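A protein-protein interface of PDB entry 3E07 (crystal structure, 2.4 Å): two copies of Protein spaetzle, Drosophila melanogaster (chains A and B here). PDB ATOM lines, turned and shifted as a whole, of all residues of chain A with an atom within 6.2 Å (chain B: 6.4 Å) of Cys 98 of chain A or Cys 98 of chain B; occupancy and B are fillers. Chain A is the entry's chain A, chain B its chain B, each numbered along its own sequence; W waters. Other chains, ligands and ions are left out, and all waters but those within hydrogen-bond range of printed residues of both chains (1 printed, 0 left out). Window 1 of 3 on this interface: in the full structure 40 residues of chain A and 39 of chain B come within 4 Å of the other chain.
The side-chain carboxylate (OE2) of Glu 45 of chain A is in salt-bridge range of the side-chain amino group (NZ) of Lys 100 of chain B, at 3.0 Å. The side-chain carboxylate (OE2) of Glu 45 of chain B lies within salt-bridge range of the side-chain amino group (NZ) of Lys 100 of chain A (3.0 Å). SG of Cys 98 of chain B is disulfide-bonded to SG of Cys 98 of chain A (2.0 Å). NZ of Lys 100 of chain A sits at hydrogen-bond distance from O of Cys 99 of chain B, at 2.7 Å. O of Cys 99 of chain A sits at hydrogen-bond distance from NZ of Lys 100 of chain B, 3.0 Å away.
OE2 of Glu 45 of chain A lies within hydrogen-bond range of N of Cys 99 of chain A, 2.8 Å away. SG of Cys 47 of chain A forms a disulfide with SG of Cys 99 of chain A. The backbone carbonyl oxygen (O) of Glu 45 of chain B is in hydrogen-bond range of the side-chain amide nitrogen (NE2) of Gln 70 of chain B (2.7 Å). The backbone NH of Lys 69 of chain B lies within hydrogen-bond range of the backbone carbonyl oxygen of Lys 100 of chain B (2.8 Å). The backbone carbonyl oxygen (O) of Pro 96 of chain A lies within hydrogen-bond range of the backbone NH (N) of Glu 45 of chain A. O of Glu 45 of chain A sits at hydrogen-bond distance from NE2 of Gln 70 of chain A (2.9 Å).
Lys 100 of chain B touches Ser 12 of chain A (NZ to OG, 3.7 Å).
Of the printed residues of chain B, Ser 12 of chain A touches Lys 100 (3.7 Å). Of chain B, only Cys 98 (2.0 Å) comes within 4 Å of Cys 98 of chain A. Cys 98 of chain B touches one residue of chain A. Of the printed residues of chain A, Lys 100 of chain B touches Ser 12 (3.7 Å), Glu 45 (3.0 Å) and Cys 99 (3.0 Å). The nearest residue of chain B that does not touch Cys 98 of chain A is Glu 45 of chain B (4.2 Å).
Printed residues of chain A that touch a printed residue of chain B: Ser 12, Glu 45, Cys 98, Cys 99 and Lys 100. Of the 14 printed residues of chain B, 4 touch a printed residue of chain A.
Ser 12 of chain A touches Lys 100 of chain B, but with the chains exchanged Lys 100 of chain A does not touch Ser 12 of chain B (4.1 Å). Glu 45 of chain A touches Lys 100 of chain B, and with the chains exchanged Lys 100 of chain A touches Glu 45 of chain B. Cys 98 of chain B touches its own counterpart, Cys 98 of chain A. Cys 99 of chain A touches Lys 100 of chain B, and with the chains exchanged Lys 100 of chain A touches Cys 99 of chain B. Of the 6 pairs that touch across the chains among the printed residues, 5 have their exchanged pair printed and touching as well.
Water W1 lies within hydrogen-bond range of the backbone carbonyl oxygen of Cys 99 of chain B and the side-chain amino group of Lys 100 of chain A.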
ATOM      1  N   SER A  12      -8.438   6.335  10.545  1.00  0.00           N
ATOM      2  CA  SER A  12      -9.337   5.201  10.705  1.00  0.00           C
ATOM      3  C   SER A  12      -9.816   4.660   9.363  1.00  0.00           C
ATOM      4  O   SER A  12      -9.740   5.341   8.339  1.00  0.00           O
ATOM      5  CB  SER A  12     -10.531   5.604  11.572  1.00  0.00           C
ATOM      6  OG  SER A  12     -11.101   6.799  11.088  1.00  0.00           O
ATOM      7  N   GLU A  45     -16.193   1.549  11.475  1.00  0.00           N
ATOM      8  CA  GLU A  45     -15.050   2.444  11.458  1.00  0.00           C
ATOM      9  C   GLU A  45     -14.031   1.968  12.477  1.00  0.00           C
ATOM     10  O   GLU A  45     -14.280   2.019  13.685  1.00  0.00           O
ATOM     11  CB  GLU A  45     -15.439   3.880  11.795  1.00  0.00           C
ATOM     12  CG  GLU A  45     -14.202   4.764  11.862  1.00  0.00           C
ATOM     13  CD  GLU A  45     -14.505   6.244  11.847  1.00  0.00           C
ATOM     14  OE1 GLU A  45     -15.175   6.698  10.894  1.00  0.00           O
ATOM     15  OE2 GLU A  45     -14.061   6.956  12.779  1.00  0.00           O
ATOM     16  N   GLU A  46     -12.886   1.506  11.993  1.00  0.00           N
ATOM     17  CA  GLU A  46     -11.821   1.029  12.872  1.00  0.00           C
ATOM     18  C   GLU A  46     -10.709   2.061  12.973  1.00  0.00           C
ATOM     19  O   GLU A  46     -10.410   2.751  11.996  1.00  0.00           O
ATOM     20  CB  GLU A  46     -11.191  -0.250  12.317  1.00  0.00           C
ATOM     21  CG  GLU A  46     -12.070  -1.469  12.266  1.00  0.00           C
ATOM     22  CD  GLU A  46     -11.342  -2.649  11.645  1.00  0.00           C
ATOM     23  OE1 GLU A  46     -11.054  -2.598  10.427  1.00  0.00           O
ATOM     24  OE2 GLU A  46     -11.039  -3.621  12.374  1.00  0.00           O
ATOM     25  N   CYS A  47     -10.086   2.166  14.141  1.00  0.00           N
ATOM     26  CA  CYS A  47      -8.957   3.076  14.291  1.00  0.00           C
ATOM     27  C   CYS A  47      -7.796   2.443  13.531  1.00  0.00           C
ATOM     28  O   CYS A  47      -7.628   1.224  13.562  1.00  0.00           O
ATOM     29  CB  CYS A  47      -8.530   3.193  15.751  1.00  0.00           C
ATOM     30  SG  CYS A  47      -9.442   4.346  16.822  1.00  0.00           S
ATOM     31  N   LYS A  69      -8.793   6.709  20.333  1.00  0.00           N
ATOM     32  CA  LYS A  69      -9.653   5.750  20.992  1.00  0.00           C
ATOM     33  C   LYS A  69     -10.717   5.156  20.085  1.00  0.00           C
ATOM     34  O   LYS A  69     -11.391   5.871  19.336  1.00  0.00           O
ATOM     35  CB  LYS A  69     -10.339   6.405  22.196  1.00  0.00           C
ATOM     36  CG  LYS A  69      -9.970   5.783  23.528  1.00  0.00           C
ATOM     37  CD  LYS A  69     -10.933   6.210  24.620  1.00  0.00           C
ATOM     38  CE  LYS A  69     -12.360   5.767  24.309  1.00  0.00           C
ATOM     39  NZ  LYS A  69     -13.324   6.151  25.374  1.00  0.00           N
ATOM     40  N   GLN A  70     -10.867   3.840  20.172  1.00  0.00           N
ATOM     41  CA  GLN A  70     -11.865   3.114  19.392  1.00  0.00           C
ATOM     42  C   GLN A  70     -13.202   3.134  20.141  1.00  0.00           C
ATOM     43  O   GLN A  70     -13.263   2.776  21.325  1.00  0.00           O
ATOM     44  CB  GLN A  70     -11.410   1.661  19.197  1.00  0.00           C
ATOM     45  CG  GLN A  70     -12.358   0.815  18.355  1.00  0.00           C
ATOM     46  CD  GLN A  70     -12.448   1.293  16.898  1.00  0.00           C
ATOM     47  OE1 GLN A  70     -11.489   1.180  16.128  1.00  0.00           O
ATOM     48  NE2 GLN A  70     -13.603   1.836  16.525  1.00  0.00           N
ATOM     49  N   HIS A  71     -14.263   3.556  19.461  1.00  0.00           N
ATOM     50  CA  HIS A  71     -15.601   3.579  20.051  1.00  0.00           C
ATOM     51  C   HIS A  71     -16.444   2.485  19.406  1.00  0.00           C
ATOM     52  O   HIS A  71     -16.188   2.087  18.267  1.00  0.00           O
ATOM     53  CB  HIS A  71     -16.267   4.936  19.829  1.00  0.00           C
ATOM     54  CG  HIS A  71     -15.760   6.012  20.736  1.00  0.00           C
ATOM     55  ND1 HIS A  71     -16.169   7.326  20.643  1.00  0.00           N
ATOM     56  CD2 HIS A  71     -14.907   5.963  21.790  1.00  0.00           C
ATOM     57  CE1 HIS A  71     -15.596   8.034  21.598  1.00  0.00           C
ATOM     58  NE2 HIS A  71     -14.825   7.228  22.308  1.00  0.00           N
ATOM     59  N   TYR A  72     -17.452   2.006  20.130  1.00  0.00           N
ATOM     60  CA  TYR A  72     -18.321   0.965  19.619  1.00  0.00           C
ATOM     61  C   TYR A  72     -19.780   1.266  19.911  1.00  0.00           C
ATOM     62  O   TYR A  72     -20.099   2.014  20.822  1.00  0.00           O
ATOM     63  CB  TYR A  72     -18.003  -0.374  20.292  1.00  0.00           C
ATOM     64  CG  TYR A  72     -16.561  -0.818  20.250  1.00  0.00           C
ATOM     65  CD1 TYR A  72     -16.099  -1.667  19.242  1.00  0.00           C
ATOM     66  CD2 TYR A  72     -15.667  -0.428  21.244  1.00  0.00           C
ATOM     67  CE1 TYR A  72     -14.791  -2.120  19.230  1.00  0.00           C
ATOM     68  CE2 TYR A  72     -14.356  -0.878  21.240  1.00  0.00           C
ATOM     69  CZ  TYR A  72     -13.925  -1.729  20.228  1.00  0.00           C
ATOM     70  OH  TYR A  72     -12.635  -2.202  20.240  1.00  0.00           O
ATOM     71  N   ILE A  95     -19.631  -3.229  17.780  1.00  0.00           N
ATOM     72  CA  ILE A  95     -19.422  -2.729  16.431  1.00  0.00           C
ATOM     73  C   ILE A  95     -18.554  -1.486  16.399  1.00  0.00           C
ATOM     74  O   ILE A  95     -18.990  -0.420  16.809  1.00  0.00           O
ATOM     75  CB  ILE A  95     -20.788  -2.408  15.785  1.00  0.00           C
ATOM     76  CG1 ILE A  95     -21.596  -3.703  15.674  1.00  0.00           C
ATOM     77  CG2 ILE A  95     -20.602  -1.713  14.433  1.00  0.00           C
ATOM     78  CD1 ILE A  95     -23.098  -3.476  15.513  1.00  0.00           C
ATOM     79  N   PRO A  96     -17.310  -1.610  15.902  1.00  0.00           N
ATOM     80  CA  PRO A  96     -16.389  -0.464  15.824  1.00  0.00           C
ATOM     81  C   PRO A  96     -17.143   0.627  15.084  1.00  0.00           C
ATOM     82  O   PRO A  96     -17.564   0.436  13.941  1.00  0.00           O
ATOM     83  CB  PRO A  96     -15.215  -1.018  15.019  1.00  0.00           C
ATOM     84  CG  PRO A  96     -15.239  -2.492  15.370  1.00  0.00           C
ATOM     85  CD  PRO A  96     -16.718  -2.803  15.275  1.00  0.00           C
ATOM     86  N   SER A  97     -17.317   1.771  15.723  1.00  0.00           N
ATOM     87  CA  SER A  97     -18.107   2.811  15.105  1.00  0.00           C
ATOM     88  C   SER A  97     -17.491   4.178  14.901  1.00  0.00           C
ATOM     89  O   SER A  97     -17.936   4.926  14.037  1.00  0.00           O
ATOM     90  CB  SER A  97     -19.398   2.982  15.911  1.00  0.00           C
ATOM     91  OG  SER A  97     -19.114   3.323  17.269  1.00  0.00           O
ATOM     92  N   CYS A  98     -16.467   4.508  15.670  1.00  0.00           N
ATOM     93  CA  CYS A  98     -15.908   5.847  15.583  1.00  0.00           C
ATOM     94  C   CYS A  98     -14.509   5.838  16.181  1.00  0.00           C
ATOM     95  O   CYS A  98     -14.280   5.243  17.225  1.00  0.00           O
ATOM     96  CB  CYS A  98     -16.854   6.756  16.387  1.00  0.00           C
ATOM     97  SG  CYS A  98     -16.692   8.569  16.473  1.00  0.00           S
ATOM     98  N   CYS A  99     -13.563   6.464  15.500  1.00  0.00           N
ATOM     99  CA  CYS A  99     -12.223   6.544  16.034  1.00  0.00           C
ATOM    100  C   CYS A  99     -12.007   8.009  16.343  1.00  0.00           C
ATOM    101  O   CYS A  99     -12.042   8.837  15.446  1.00  0.00           O
ATOM    102  CB  CYS A  99     -11.179   6.066  15.026  1.00  0.00           C
ATOM    103  SG  CYS A  99      -9.525   6.095  15.786  1.00  0.00           S
ATOM    104  N   LYS A 100     -11.811   8.349  17.607  1.00  0.00           N
ATOM    105  CA  LYS A 100     -11.596   9.745  17.950  1.00  0.00           C
ATOM    106  C   LYS A 100     -10.527   9.938  19.015  1.00  0.00           C
ATOM    107  O   LYS A 100     -10.161   9.001  19.740  1.00  0.00           O
ATOM    108  CB  LYS A 100     -12.912  10.402  18.380  1.00  0.00           C
ATOM    109  CG  LYS A 100     -13.586   9.777  19.567  1.00  0.00           C
ATOM    110  CD  LYS A 100     -14.731  10.664  20.081  1.00  0.00           C
ATOM    111  CE  LYS A 100     -15.879  10.790  19.088  1.00  0.00           C
ATOM    112  NZ  LYS A 100     -16.994  11.630  19.638  1.00  0.00           N
ATOM    113  N   SER B  12     -20.842  15.845  22.221  1.00  0.00           N
ATOM    114  CA  SER B  12     -21.837  15.136  21.434  1.00  0.00           C
ATOM    115  C   SER B  12     -22.791  14.449  22.382  1.00  0.00           C
ATOM    116  O   SER B  12     -22.525  14.345  23.574  1.00  0.00           O
ATOM    117  CB  SER B  12     -21.161  14.101  20.528  1.00  0.00           C
ATOM    118  OG  SER B  12     -20.459  13.144  21.304  1.00  0.00           O
ATOM    119  N   GLU B  45     -25.221   8.987  17.876  1.00  0.00           N
ATOM    120  CA  GLU B  45     -24.375   9.994  18.508  1.00  0.00           C
ATOM    121  C   GLU B  45     -24.466  11.261  17.683  1.00  0.00           C
ATOM    122  O   GLU B  45     -24.057  11.277  16.525  1.00  0.00           O
ATOM    123  CB  GLU B  45     -22.916   9.553  18.575  1.00  0.00           C
ATOM    124  CG  GLU B  45     -21.976  10.711  18.932  1.00  0.00           C
ATOM    125  CD  GLU B  45     -20.589  10.254  19.334  1.00  0.00           C
ATOM    126  OE1 GLU B  45     -20.475   9.511  20.332  1.00  0.00           O
ATOM    127  OE2 GLU B  45     -19.610  10.637  18.661  1.00  0.00           O
ATOM    128  N   GLU B  46     -25.010  12.318  18.278  1.00  0.00           N
ATOM    129  CA  GLU B  46     -25.163  13.586  17.573  1.00  0.00           C
ATOM    130  C   GLU B  46     -24.271  14.690  18.124  1.00  0.00           C
ATOM    131  O   GLU B  46     -24.056  14.796  19.336  1.00  0.00           O
ATOM    132  CB  GLU B  46     -26.615  14.044  17.639  1.00  0.00           C
ATOM    133  CG  GLU B  46     -27.577  13.187  16.855  1.00  0.00           C
ATOM    134  CD  GLU B  46     -29.017  13.409  17.279  1.00  0.00           C
ATOM    135  OE1 GLU B  46     -29.932  13.061  16.500  1.00  0.00           O
ATOM    136  OE2 GLU B  46     -29.233  13.922  18.400  1.00  0.00           O
ATOM    137  N   CYS B  47     -23.754  15.511  17.220  1.00  0.00           N
ATOM    138  CA  CYS B  47     -22.901  16.631  17.600  1.00  0.00           C
ATOM    139  C   CYS B  47     -23.767  17.675  18.291  1.00  0.00           C
ATOM    140  O   CYS B  47     -24.721  18.188  17.700  1.00  0.00           O
ATOM    141  CB  CYS B  47     -22.267  17.281  16.368  1.00  0.00           C
ATOM    142  SG  CYS B  47     -20.701  16.623  15.690  1.00  0.00           S
ATOM    143  N   LYS B  69     -17.505  17.813  13.242  1.00  0.00           N
ATOM    144  CA  LYS B  69     -18.273  17.235  12.143  1.00  0.00           C
ATOM    145  C   LYS B  69     -19.110  16.034  12.529  1.00  0.00           C
ATOM    146  O   LYS B  69     -18.640  15.132  13.227  1.00  0.00           O
ATOM    147  CB  LYS B  69     -17.335  16.824  11.017  1.00  0.00           C
ATOM    148  CG  LYS B  69     -16.910  17.958  10.137  1.00  0.00           C
ATOM    149  CD  LYS B  69     -18.107  18.494   9.382  1.00  0.00           C
ATOM    150  CE  LYS B  69     -17.713  19.630   8.462  1.00  0.00           C
ATOM    151  NZ  LYS B  69     -18.872  20.050   7.633  1.00  0.00           N
ATOM    152  N   GLN B  70     -20.350  16.026  12.054  1.00  0.00           N
ATOM    153  CA  GLN B  70     -21.280  14.939  12.313  1.00  0.00           C
ATOM    154  C   GLN B  70     -21.144  13.895  11.210  1.00  0.00           C
ATOM    155  O   GLN B  70     -21.104  14.242  10.037  1.00  0.00           O
ATOM    156  CB  GLN B  70     -22.710  15.466  12.320  1.00  0.00           C
ATOM    157  CG  GLN B  70     -23.756  14.393  12.486  1.00  0.00           C
ATOM    158  CD  GLN B  70     -23.959  14.000  13.932  1.00  0.00           C
ATOM    159  OE1 GLN B  70     -24.472  14.785  14.731  1.00  0.00           O
ATOM    160  NE2 GLN B  70     -23.560  12.782  14.278  1.00  0.00           N
ATOM    161  N   HIS B  71     -21.075  12.623  11.590  1.00  0.00           N
ATOM    162  CA  HIS B  71     -20.967  11.544  10.618  1.00  0.00           C
ATOM    163  C   HIS B  71     -22.159  10.613  10.723  1.00  0.00           C
ATOM    164  O   HIS B  71     -22.776  10.507  11.776  1.00  0.00           O
ATOM    165  CB  HIS B  71     -19.680  10.760  10.828  1.00  0.00           C
ATOM    166  CG  HIS B  71     -18.448  11.541  10.520  1.00  0.00           C
ATOM    167  ND1 HIS B  71     -18.278  12.219   9.327  1.00  0.00           N
ATOM    168  CD2 HIS B  71     -17.324  11.759  11.231  1.00  0.00           C
ATOM    169  CE1 HIS B  71     -17.106  12.815   9.326  1.00  0.00           C
ATOM    170  NE2 HIS B  71     -16.500  12.552  10.472  1.00  0.00           N
ATOM    171  N   TYR B  72     -22.474   9.933   9.629  1.00  0.00           N
ATOM    172  CA  TYR B  72     -23.609   9.026   9.608  1.00  0.00           C
ATOM    173  C   TYR B  72     -23.240   7.673   9.033  1.00  0.00           C
ATOM    174  O   TYR B  72     -22.237   7.529   8.340  1.00  0.00           O
ATOM    175  CB  TYR B  72     -24.717   9.615   8.740  1.00  0.00           C
ATOM    176  CG  TYR B  72     -25.104  11.022   9.084  1.00  0.00           C
ATOM    177  CD1 TYR B  72     -26.130  11.276   9.997  1.00  0.00           C
ATOM    178  CD2 TYR B  72     -24.444  12.102   8.505  1.00  0.00           C
ATOM    179  CE1 TYR B  72     -26.494  12.578  10.328  1.00  0.00           C
ATOM    180  CE2 TYR B  72     -24.798  13.414   8.827  1.00  0.00           C
ATOM    181  CZ  TYR B  72     -25.825  13.641   9.740  1.00  0.00           C
ATOM    182  OH  TYR B  72     -26.177  14.930  10.078  1.00  0.00           O
ATOM    183  N   ILE B  95     -28.117   7.640   9.867  1.00  0.00           N
ATOM    184  CA  ILE B  95     -28.051   7.444  11.301  1.00  0.00           C
ATOM    185  C   ILE B  95     -26.838   8.162  11.870  1.00  0.00           C
ATOM    186  O   ILE B  95     -25.699   7.816  11.558  1.00  0.00           O
ATOM    187  CB  ILE B  95     -27.961   5.939  11.620  1.00  0.00           C
ATOM    188  CG1 ILE B  95     -29.260   5.265  11.180  1.00  0.00           C
ATOM    189  CG2 ILE B  95     -27.667   5.713  13.095  1.00  0.00           C
ATOM    190  CD1 ILE B  95     -29.122   3.799  10.921  1.00  0.00           C
ATOM    191  N   PRO B  96     -27.067   9.183  12.706  1.00  0.00           N
ATOM    192  CA  PRO B  96     -25.956   9.929  13.305  1.00  0.00           C
ATOM    193  C   PRO B  96     -25.083   8.922  14.046  1.00  0.00           C
ATOM    194  O   PRO B  96     -25.582   8.190  14.905  1.00  0.00           O
ATOM    195  CB  PRO B  96     -26.660  10.892  14.257  1.00  0.00           C
ATOM    196  CG  PRO B  96     -28.018  11.073  13.620  1.00  0.00           C
ATOM    197  CD  PRO B  96     -28.361   9.668  13.217  1.00  0.00           C
ATOM    198  N   SER B  97     -23.790   8.878  13.740  1.00  0.00           N
ATOM    199  CA  SER B  97     -22.959   7.881  14.392  1.00  0.00           C
ATOM    200  C   SER B  97     -21.664   8.327  15.050  1.00  0.00           C
ATOM    201  O   SER B  97     -21.210   7.702  16.000  1.00  0.00           O
ATOM    202  CB  SER B  97     -22.640   6.760  13.390  1.00  0.00           C
ATOM    203  OG  SER B  97     -21.962   7.259  12.242  1.00  0.00           O
ATOM    204  N   CYS B  98     -21.078   9.412  14.570  1.00  0.00           N
ATOM    205  CA  CYS B  98     -19.782   9.831  15.087  1.00  0.00           C
ATOM    206  C   CYS B  98     -19.626  11.344  15.012  1.00  0.00           C
ATOM    207  O   CYS B  98     -19.830  11.943  13.951  1.00  0.00           O
ATOM    208  CB  CYS B  98     -18.722   9.135  14.216  1.00  0.00           C
ATOM    209  SG  CYS B  98     -16.922   9.195  14.557  1.00  0.00           S
ATOM    210  N   CYS B  99     -19.281  11.965  16.136  1.00  0.00           N
ATOM    211  CA  CYS B  99     -19.054  13.406  16.160  1.00  0.00           C
ATOM    212  C   CYS B  99     -17.574  13.605  16.484  1.00  0.00           C
ATOM    213  O   CYS B  99     -17.153  13.478  17.630  1.00  0.00           O
ATOM    214  CB  CYS B  99     -19.940  14.105  17.213  1.00  0.00           C
ATOM    215  SG  CYS B  99     -19.637  15.902  17.268  1.00  0.00           S
ATOM    216  N   LYS B 100     -16.779  13.907  15.466  1.00  0.00           N
ATOM    217  CA  LYS B 100     -15.350  14.084  15.671  1.00  0.00           C
ATOM    218  C   LYS B 100     -14.862  15.403  15.103  1.00  0.00           C
ATOM    219  O   LYS B 100     -15.571  16.040  14.325  1.00  0.00           O
ATOM    220  CB  LYS B 100     -14.593  12.903  15.048  1.00  0.00           C
ATOM    221  CG  LYS B 100     -15.019  12.582  13.626  1.00  0.00           C
ATOM    222  CD  LYS B 100     -14.615  11.173  13.211  1.00  0.00           C
ATOM    223  CE  LYS B 100     -13.114  10.968  13.238  1.00  0.00           C
ATOM    224  NZ  LYS B 100     -12.771   9.635  12.688  1.00  0.00           N
HETATM  225  O   HOH W   1     -15.276  14.369  20.161  1.00  0.00           O
